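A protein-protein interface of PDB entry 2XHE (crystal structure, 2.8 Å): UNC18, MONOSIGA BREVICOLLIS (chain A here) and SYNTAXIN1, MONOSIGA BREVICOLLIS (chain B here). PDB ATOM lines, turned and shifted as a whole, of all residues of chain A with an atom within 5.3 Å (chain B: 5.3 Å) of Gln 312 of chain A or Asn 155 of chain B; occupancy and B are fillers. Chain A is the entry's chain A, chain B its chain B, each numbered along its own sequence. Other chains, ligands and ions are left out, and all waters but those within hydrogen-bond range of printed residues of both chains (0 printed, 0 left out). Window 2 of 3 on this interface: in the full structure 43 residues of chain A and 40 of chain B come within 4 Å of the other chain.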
ATOM      1  N   ALA A 308     -16.656  29.308 -28.522  1.00  0.00           N
ATOM      2  CA  ALA A 308     -15.768  28.276 -28.006  1.00  0.00           C
ATOM      3  C   ALA A 308     -15.019  27.594 -29.132  1.00  0.00           C
ATOM      4  O   ALA A 308     -14.012  26.937 -28.904  1.00  0.00           O
ATOM      5  CB  ALA A 308     -16.526  27.269 -27.188  1.00  0.00           C
ATOM      6  N   ARG A 309     -15.511  27.759 -30.352  1.00  0.00           N
ATOM      7  CA  ARG A 309     -14.786  27.266 -31.511  1.00  0.00           C
ATOM      8  C   ARG A 309     -13.713  28.252 -31.977  1.00  0.00           C
ATOM      9  O   ARG A 309     -12.665  27.844 -32.471  1.00  0.00           O
ATOM     10  CB  ARG A 309     -15.750  26.910 -32.640  1.00  0.00           C
ATOM     11  CG  ARG A 309     -16.480  25.624 -32.369  1.00  0.00           C
ATOM     12  CD  ARG A 309     -17.372  25.210 -33.509  1.00  0.00           C
ATOM     13  NE  ARG A 309     -17.469  23.758 -33.573  1.00  0.00           N
ATOM     14  CZ  ARG A 309     -16.852  23.025 -34.495  1.00  0.00           C
ATOM     15  NH1 ARG A 309     -16.129  23.617 -35.440  1.00  0.00           N
ATOM     16  NH2 ARG A 309     -16.969  21.704 -34.487  1.00  0.00           N
ATOM     17  N   ARG A 310     -13.967  29.546 -31.804  1.00  0.00           N
ATOM     18  CA  ARG A 310     -12.993  30.558 -32.202  1.00  0.00           C
ATOM     19  C   ARG A 310     -11.841  30.651 -31.209  1.00  0.00           C
ATOM     20  O   ARG A 310     -10.795  31.210 -31.522  1.00  0.00           O
ATOM     21  CB  ARG A 310     -13.651  31.927 -32.394  1.00  0.00           C
ATOM     22  CG  ARG A 310     -14.528  32.046 -33.634  1.00  0.00           C
ATOM     23  CD  ARG A 310     -15.211  33.411 -33.671  1.00  0.00           C
ATOM     24  NE  ARG A 310     -16.325  33.467 -34.619  1.00  0.00           N
ATOM     25  CZ  ARG A 310     -17.319  34.350 -34.552  1.00  0.00           C
ATOM     26  NH1 ARG A 310     -17.345  35.250 -33.573  1.00  0.00           N
ATOM     27  NH2 ARG A 310     -18.294  34.330 -35.456  1.00  0.00           N
ATOM     28  N   LEU A 311     -12.035  30.107 -30.012  1.00  0.00           N
ATOM     29  CA  LEU A 311     -10.944  30.012 -29.048  1.00  0.00           C
ATOM     30  C   LEU A 311      -9.958  28.956 -29.497  1.00  0.00           C
ATOM     31  O   LEU A 311      -8.769  29.080 -29.243  1.00  0.00           O
ATOM     32  CB  LEU A 311     -11.452  29.700 -27.643  1.00  0.00           C
ATOM     33  CG  LEU A 311     -12.135  30.858 -26.916  1.00  0.00           C
ATOM     34  CD1 LEU A 311     -12.466  30.455 -25.485  1.00  0.00           C
ATOM     35  CD2 LEU A 311     -11.260  32.101 -26.936  1.00  0.00           C
ATOM     36  N   GLN A 312     -10.447  27.915 -30.160  1.00  0.00           N
ATOM     37  CA  GLN A 312      -9.557  27.018 -30.892  1.00  0.00           C
ATOM     38  C   GLN A 312      -9.397  27.510 -32.338  1.00  0.00           C
ATOM     39  O   GLN A 312      -9.030  28.664 -32.573  1.00  0.00           O
ATOM     40  CB  GLN A 312     -10.080  25.583 -30.872  1.00  0.00           C
ATOM     41  CG  GLN A 312      -9.147  24.601 -30.198  1.00  0.00           C
ATOM     42  CD  GLN A 312      -9.680  24.169 -28.862  1.00  0.00           C
ATOM     43  OE1 GLN A 312     -10.738  24.626 -28.445  1.00  0.00           O
ATOM     44  NE2 GLN A 312      -8.965  23.285 -28.184  1.00  0.00           N
ATOM     45  N   GLY A 313      -9.684  26.642 -33.302  1.00  0.00           N
ATOM     46  CA  GLY A 313      -9.601  27.012 -34.702  1.00  0.00           C
ATOM     47  C   GLY A 313     -10.513  26.156 -35.554  1.00  0.00           C
ATOM     48  O   GLY A 313     -10.098  25.122 -36.075  1.00  0.00           O
ATOM     49  N   LEU A 314     -11.757  26.596 -35.708  1.00  0.00           N
ATOM     50  CA  LEU A 314     -12.766  25.813 -36.407  1.00  0.00           C
ATOM     51  C   LEU A 314     -13.834  26.765 -36.987  1.00  0.00           C
ATOM     52  O   LEU A 314     -13.603  27.972 -37.048  1.00  0.00           O
ATOM     53  CB  LEU A 314     -13.366  24.794 -35.426  1.00  0.00           C
ATOM     54  CG  LEU A 314     -12.404  23.846 -34.676  1.00  0.00           C
ATOM     55  CD1 LEU A 314     -12.812  23.594 -33.226  1.00  0.00           C
ATOM     56  CD2 LEU A 314     -12.251  22.521 -35.413  1.00  0.00           C
ATOM     57  N   LEU A 334     -15.208  19.512 -28.455  1.00  0.00           N
ATOM     58  CA  LEU A 334     -14.704  20.207 -27.277  1.00  0.00           C
ATOM     59  C   LEU A 334     -15.159  19.542 -25.971  1.00  0.00           C
ATOM     60  O   LEU A 334     -15.879  20.152 -25.172  1.00  0.00           O
ATOM     61  CB  LEU A 334     -15.180  21.662 -27.296  1.00  0.00           C
ATOM     62  CG  LEU A 334     -14.387  22.715 -28.078  1.00  0.00           C
ATOM     63  CD1 LEU A 334     -13.272  22.079 -28.879  1.00  0.00           C
ATOM     64  CD2 LEU A 334     -15.306  23.557 -28.971  1.00  0.00           C
ATOM     65  N   GLN A 336     -13.828  19.167 -23.239  1.00  0.00           N
ATOM     66  CA  GLN A 336     -13.548  20.114 -22.160  1.00  0.00           C
ATOM     67  C   GLN A 336     -14.810  20.798 -21.631  1.00  0.00           C
ATOM     68  O   GLN A 336     -14.958  21.025 -20.432  1.00  0.00           O
ATOM     69  CB  GLN A 336     -12.600  21.178 -22.696  1.00  0.00           C
ATOM     70  CG  GLN A 336     -12.454  21.070 -24.201  1.00  0.00           C
ATOM     71  CD  GLN A 336     -11.752  22.246 -24.801  1.00  0.00           C
ATOM     72  OE1 GLN A 336     -11.303  22.189 -25.942  1.00  0.00           O
ATOM     73  NE2 GLN A 336     -11.640  23.331 -24.034  1.00  0.00           N
ATOM     74  N   MET B 151      -6.575  21.624 -16.588  1.00  0.00           N
ATOM     75  CA  MET B 151      -6.096  21.361 -17.934  1.00  0.00           C
ATOM     76  C   MET B 151      -6.791  22.253 -18.941  1.00  0.00           C
ATOM     77  O   MET B 151      -6.260  22.538 -20.007  1.00  0.00           O
ATOM     78  CB  MET B 151      -6.270  19.891 -18.304  1.00  0.00           C
ATOM     79  CG  MET B 151      -5.384  18.974 -17.472  1.00  0.00           C
ATOM     80  SD  MET B 151      -3.676  19.583 -17.310  1.00  0.00           S
ATOM     81  CE  MET B 151      -2.922  18.852 -18.765  1.00  0.00           C
ATOM     82  N   THR B 152      -7.986  22.700 -18.598  1.00  0.00           N
ATOM     83  CA  THR B 152      -8.730  23.548 -19.501  1.00  0.00           C
ATOM     84  C   THR B 152      -8.048  24.897 -19.546  1.00  0.00           C
ATOM     85  O   THR B 152      -8.055  25.568 -20.574  1.00  0.00           O
ATOM     86  CB  THR B 152     -10.196  23.685 -19.068  1.00  0.00           C
ATOM     87  OG1 THR B 152     -10.841  22.415 -19.217  1.00  0.00           O
ATOM     88  CG2 THR B 152     -10.919  24.710 -19.925  1.00  0.00           C
ATOM     89  N   ARG B 153      -7.448  25.285 -18.426  1.00  0.00           N
ATOM     90  CA  ARG B 153      -6.694  26.531 -18.378  1.00  0.00           C
ATOM     91  C   ARG B 153      -5.496  26.400 -19.310  1.00  0.00           C
ATOM     92  O   ARG B 153      -5.188  27.316 -20.068  1.00  0.00           O
ATOM     93  CB  ARG B 153      -6.258  26.858 -16.950  1.00  0.00           C
ATOM     94  CG  ARG B 153      -5.413  28.112 -16.833  1.00  0.00           C
ATOM     95  CD  ARG B 153      -6.020  29.274 -17.607  1.00  0.00           C
ATOM     96  NE  ARG B 153      -5.183  30.472 -17.532  1.00  0.00           N
ATOM     97  CZ  ARG B 153      -5.192  31.457 -18.428  1.00  0.00           C
ATOM     98  NH1 ARG B 153      -5.994  31.394 -19.486  1.00  0.00           N
ATOM     99  NH2 ARG B 153      -4.392  32.505 -18.269  1.00  0.00           N
ATOM    100  N   TYR B 154      -4.848  25.238 -19.264  1.00  0.00           N
ATOM    101  CA  TYR B 154      -3.737  24.918 -20.157  1.00  0.00           C
ATOM    102  C   TYR B 154      -4.193  24.951 -21.616  1.00  0.00           C
ATOM    103  O   TYR B 154      -3.649  25.693 -22.430  1.00  0.00           O
ATOM    104  CB  TYR B 154      -3.169  23.542 -19.801  1.00  0.00           C
ATOM    105  CG  TYR B 154      -1.892  23.153 -20.519  1.00  0.00           C
ATOM    106  CD1 TYR B 154      -0.782  23.987 -20.519  1.00  0.00           C
ATOM    107  CD2 TYR B 154      -1.786  21.924 -21.164  1.00  0.00           C
ATOM    108  CE1 TYR B 154       0.397  23.617 -21.168  1.00  0.00           C
ATOM    109  CE2 TYR B 154      -0.615  21.543 -21.812  1.00  0.00           C
ATOM    110  CZ  TYR B 154       0.475  22.391 -21.812  1.00  0.00           C
ATOM    111  OH  TYR B 154       1.635  22.010 -22.459  1.00  0.00           O
ATOM    112  N   ASN B 155      -5.199  24.148 -21.941  1.00  0.00           N
ATOM    113  CA  ASN B 155      -5.753  24.123 -23.290  1.00  0.00           C
ATOM    114  C   ASN B 155      -6.056  25.528 -23.804  1.00  0.00           C
ATOM    115  O   ASN B 155      -5.904  25.806 -24.996  1.00  0.00           O
ATOM    116  CB  ASN B 155      -7.016  23.253 -23.331  1.00  0.00           C
ATOM    117  CG  ASN B 155      -7.642  23.187 -24.712  1.00  0.00           C
ATOM    118  OD1 ASN B 155      -8.447  24.049 -25.085  1.00  0.00           O
ATOM    119  ND2 ASN B 155      -7.300  22.143 -25.472  1.00  0.00           N
ATOM    120  N   ASP B 156      -6.471  26.414 -22.902  1.00  0.00           N
ATOM    121  CA  ASP B 156      -6.854  27.765 -23.297  1.00  0.00           C
ATOM    122  C   ASP B 156      -5.655  28.644 -23.620  1.00  0.00           C
ATOM    123  O   ASP B 156      -5.697  29.398 -24.586  1.00  0.00           O
ATOM    124  CB  ASP B 156      -7.744  28.423 -22.241  1.00  0.00           C
ATOM    125  CG  ASP B 156      -9.229  28.204 -22.509  1.00  0.00           C
ATOM    126  OD1 ASP B 156      -9.580  27.657 -23.582  1.00  0.00           O
ATOM    127  OD2 ASP B 156     -10.049  28.587 -21.647  1.00  0.00           O
ATOM    128  N   VAL B 157      -4.589  28.539 -22.825  1.00  0.00           N
ATOM    129  CA  VAL B 157      -3.367  29.318 -23.065  1.00  0.00           C
ATOM    130  C   VAL B 157      -2.594  28.822 -24.294  1.00  0.00           C
ATOM    131  O   VAL B 157      -1.934  29.608 -24.972  1.00  0.00           O
ATOM    132  CB  VAL B 157      -2.447  29.376 -21.813  1.00  0.00           C
ATOM    133  CG1 VAL B 157      -2.175  27.990 -21.284  1.00  0.00           C
ATOM    134  CG2 VAL B 157      -1.137  30.093 -22.126  1.00  0.00           C
ATOM    135  N   GLN B 158      -2.690  27.527 -24.589  1.00  0.00           N
ATOM    136  CA  GLN B 158      -2.075  26.972 -25.800  1.00  0.00           C
ATOM    137  C   GLN B 158      -2.747  27.475 -27.078  1.00  0.00           C
ATOM    138  O   GLN B 158      -2.106  28.098 -27.922  1.00  0.00           O
ATOM    139  CB  GLN B 158      -2.058  25.438 -25.768  1.00  0.00           C
ATOM    140  CG  GLN B 158      -1.116  24.838 -24.718  1.00  0.00           C
ATOM    141  CD  GLN B 158       0.365  25.159 -24.964  1.00  0.00           C
ATOM    142  OE1 GLN B 158       1.122  24.322 -25.455  1.00  0.00           O
ATOM    143  NE2 GLN B 158       0.776  26.368 -24.607  1.00  0.00           N
ATOM    144  N   ALA B 159      -4.036  27.207 -27.223  1.00  0.00           N
ATOM    145  CA  ALA B 159      -4.785  27.707 -28.371  1.00  0.00           C
ATOM    146  C   ALA B 159      -4.783  29.235 -28.444  1.00  0.00           C
ATOM    147  O   ALA B 159      -4.724  29.804 -29.530  1.00  0.00           O
ATOM    148  CB  ALA B 159      -6.201  27.183 -28.342  1.00  0.00           C
ATOM    149  N   GLU B 160      -4.854  29.887 -27.286  1.00  0.00           N
ATOM    150  CA  GLU B 160      -4.798  31.348 -27.202  1.00  0.00           C
ATOM    151  C   GLU B 160      -3.526  31.881 -27.841  1.00  0.00           C
ATOM    152  O   GLU B 160      -3.562  32.851 -28.599  1.00  0.00           O
ATOM    153  CB  GLU B 160      -4.872  31.799 -25.739  1.00  0.00           C
ATOM    154  CG  GLU B 160      -4.687  33.294 -25.492  1.00  0.00           C
ATOM    155  CD  GLU B 160      -4.912  33.679 -24.026  1.00  0.00           C
ATOM    156  OE1 GLU B 160      -4.302  34.667 -23.566  1.00  0.00           O
ATOM    157  OE2 GLU B 160      -5.697  32.993 -23.330  1.00  0.00           O
ATOM    158  N   ARG B 163      -3.082  30.992 -31.820  1.00  0.00           N
ATOM    159  CA  ARG B 163      -3.860  31.860 -32.695  1.00  0.00           C
ATOM    160  C   ARG B 163      -3.081  33.136 -33.015  1.00  0.00           C
ATOM    161  O   ARG B 163      -3.081  33.599 -34.155  1.00  0.00           O
ATOM    162  CB  ARG B 163      -5.218  32.184 -32.060  1.00  0.00           C
ATOM    163  CG  ARG B 163      -6.057  33.206 -32.815  1.00  0.00           C
ATOM    164  CD  ARG B 163      -7.534  33.137 -32.411  1.00  0.00           C
ATOM    165  NE  ARG B 163      -7.723  32.780 -31.004  1.00  0.00           N
ATOM    166  CZ  ARG B 163      -7.523  33.608 -29.982  1.00  0.00           C
ATOM    167  NH1 ARG B 163      -7.109  34.852 -30.197  1.00  0.00           N
ATOM    168  NH2 ARG B 163      -7.724  33.188 -28.741  1.00  0.00           N
ATOM    169  N   LEU B 226      -2.579  20.565 -28.164  1.00  0.00           N
ATOM    170  CA  LEU B 226      -4.038  20.587 -28.240  1.00  0.00           C
ATOM    171  C   LEU B 226      -4.617  19.198 -28.514  1.00  0.00           C
ATOM    172  O   LEU B 226      -5.699  18.858 -28.034  1.00  0.00           O
ATOM    173  CB  LEU B 226      -4.505  21.587 -29.297  1.00  0.00           C
ATOM    174  CG  LEU B 226      -4.136  23.043 -29.000  1.00  0.00           C
ATOM    175  CD1 LEU B 226      -4.352  23.910 -30.224  1.00  0.00           C
ATOM    176  CD2 LEU B 226      -4.913  23.588 -27.806  1.00  0.00           C
ATOM    177  N   LEU B 229      -4.327  17.002 -25.229  1.00  0.00           N
ATOM    178  CA  LEU B 229      -5.391  17.540 -24.398  1.00  0.00           C
ATOM    179  C   LEU B 229      -6.767  17.060 -24.845  1.00  0.00           C
ATOM    180  O   LEU B 229      -7.520  16.501 -24.043  1.00  0.00           O
ATOM    181  CB  LEU B 229      -5.346  19.062 -24.433  1.00  0.00           C
ATOM    182  CG  LEU B 229      -4.136  19.648 -23.714  1.00  0.00           C
ATOM    183  CD1 LEU B 229      -4.154  21.164 -23.806  1.00  0.00           C
ATOM    184  CD2 LEU B 229      -4.110  19.173 -22.258  1.00  0.00           C
ATOM    185  N   HIS B 230      -7.090  17.284 -26.118  1.00  0.00           N
ATOM    186  CA  HIS B 230      -8.333  16.775 -26.688  1.00  0.00           C
ATOM    187  C   HIS B 230      -8.535  15.295 -26.392  1.00  0.00           C
ATOM    188  O   HIS B 230      -9.580  14.891 -25.883  1.00  0.00           O
ATOM    189  CB  HIS B 230      -8.386  17.003 -28.195  1.00  0.00           C
ATOM    190  CG  HIS B 230      -9.619  16.453 -28.837  1.00  0.00           C
ATOM    191  ND1 HIS B 230     -10.698  17.243 -29.169  1.00  0.00           N
ATOM    192  CD2 HIS B 230      -9.956  15.188 -29.181  1.00  0.00           C
ATOM    193  CE1 HIS B 230     -11.643  16.488 -29.700  1.00  0.00           C
ATOM    194  NE2 HIS B 230     -11.218  15.237 -29.717  1.00  0.00           N
ATOM    195  N   PHE B 233      -9.275  15.103 -22.614  1.00  0.00           N
ATOM    196  CA  PHE B 233     -10.612  15.589 -22.326  1.00  0.00           C
ATOM    197  C   PHE B 233     -11.661  14.585 -22.785  1.00  0.00           C
ATOM    198  O   PHE B 233     -12.692  14.410 -22.130  1.00  0.00           O
ATOM    199  CB  PHE B 233     -10.852  16.943 -22.993  1.00  0.00           C
ATOM    200  CG  PHE B 233     -10.117  18.087 -22.342  1.00  0.00           C
ATOM    201  CD1 PHE B 233     -10.172  18.282 -20.970  1.00  0.00           C
ATOM    202  CD2 PHE B 233      -9.405  18.991 -23.109  1.00  0.00           C
ATOM    203  CE1 PHE B 233      -9.520  19.342 -20.380  1.00  0.00           C
ATOM    204  CE2 PHE B 233      -8.758  20.047 -22.529  1.00  0.00           C
ATOM    205  CZ  PHE B 233      -8.808  20.220 -21.158  1.00  0.00           C
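Of the 15 printed residues of chain B, 4 touch a printed residue of chain A.
Of the 9 printed residues of chain A, 4 touch a printed residue of chain B.
NE2 of Gln 312 of chain A is in hydrogen-bond range of OE1 of Gln 336 of chain A (3.4 Å).
The backbone carbonyl oxygen (O) of Arg 310 of chain A sits at hydrogen-bond distance from the guanidinium group (NE) of Arg 163 of chain B (3.5 Å).
OD1 of Asn 155 of chain B is in hydrogen-bond range of NE2 of Gln 312 of chain A.
The side-chain amide oxygen (OD1) of Asn 155 of chain B sits at hydrogen-bond distance from the side-chain amide nitrogen (NE2) of Gln 336 of chain A.
CB of Ala 159 of chain B touches O of Leu 311 of chain A (3.3 Å).
Phe 233 of chain B touches Gln 336 of chain A (CB to N, 3.7 Å).
Of the printed residues of chain B, Leu 311 of chain A touches Ala 159 (3.3 Å).
Of the printed residues of chain B, Gln 312 of chain A touches Asn 155 (3.2 Å).
Leu 334 of chain A touches none of the printed residues of chain B.
Asn 155 of chain B touches two residues of chain A.
Printed residues of chain A within 4 Å of Ala 159 of chain B: Leu 311.
The nearest printed residue of chain A that does not touch Asn 155 of chain B is Leu 311 of chain A (6.1 Å).
The nearest printed residue of chain B that does not touch Leu 311 of chain A is Arg 163 of chain B (4.1 Å).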
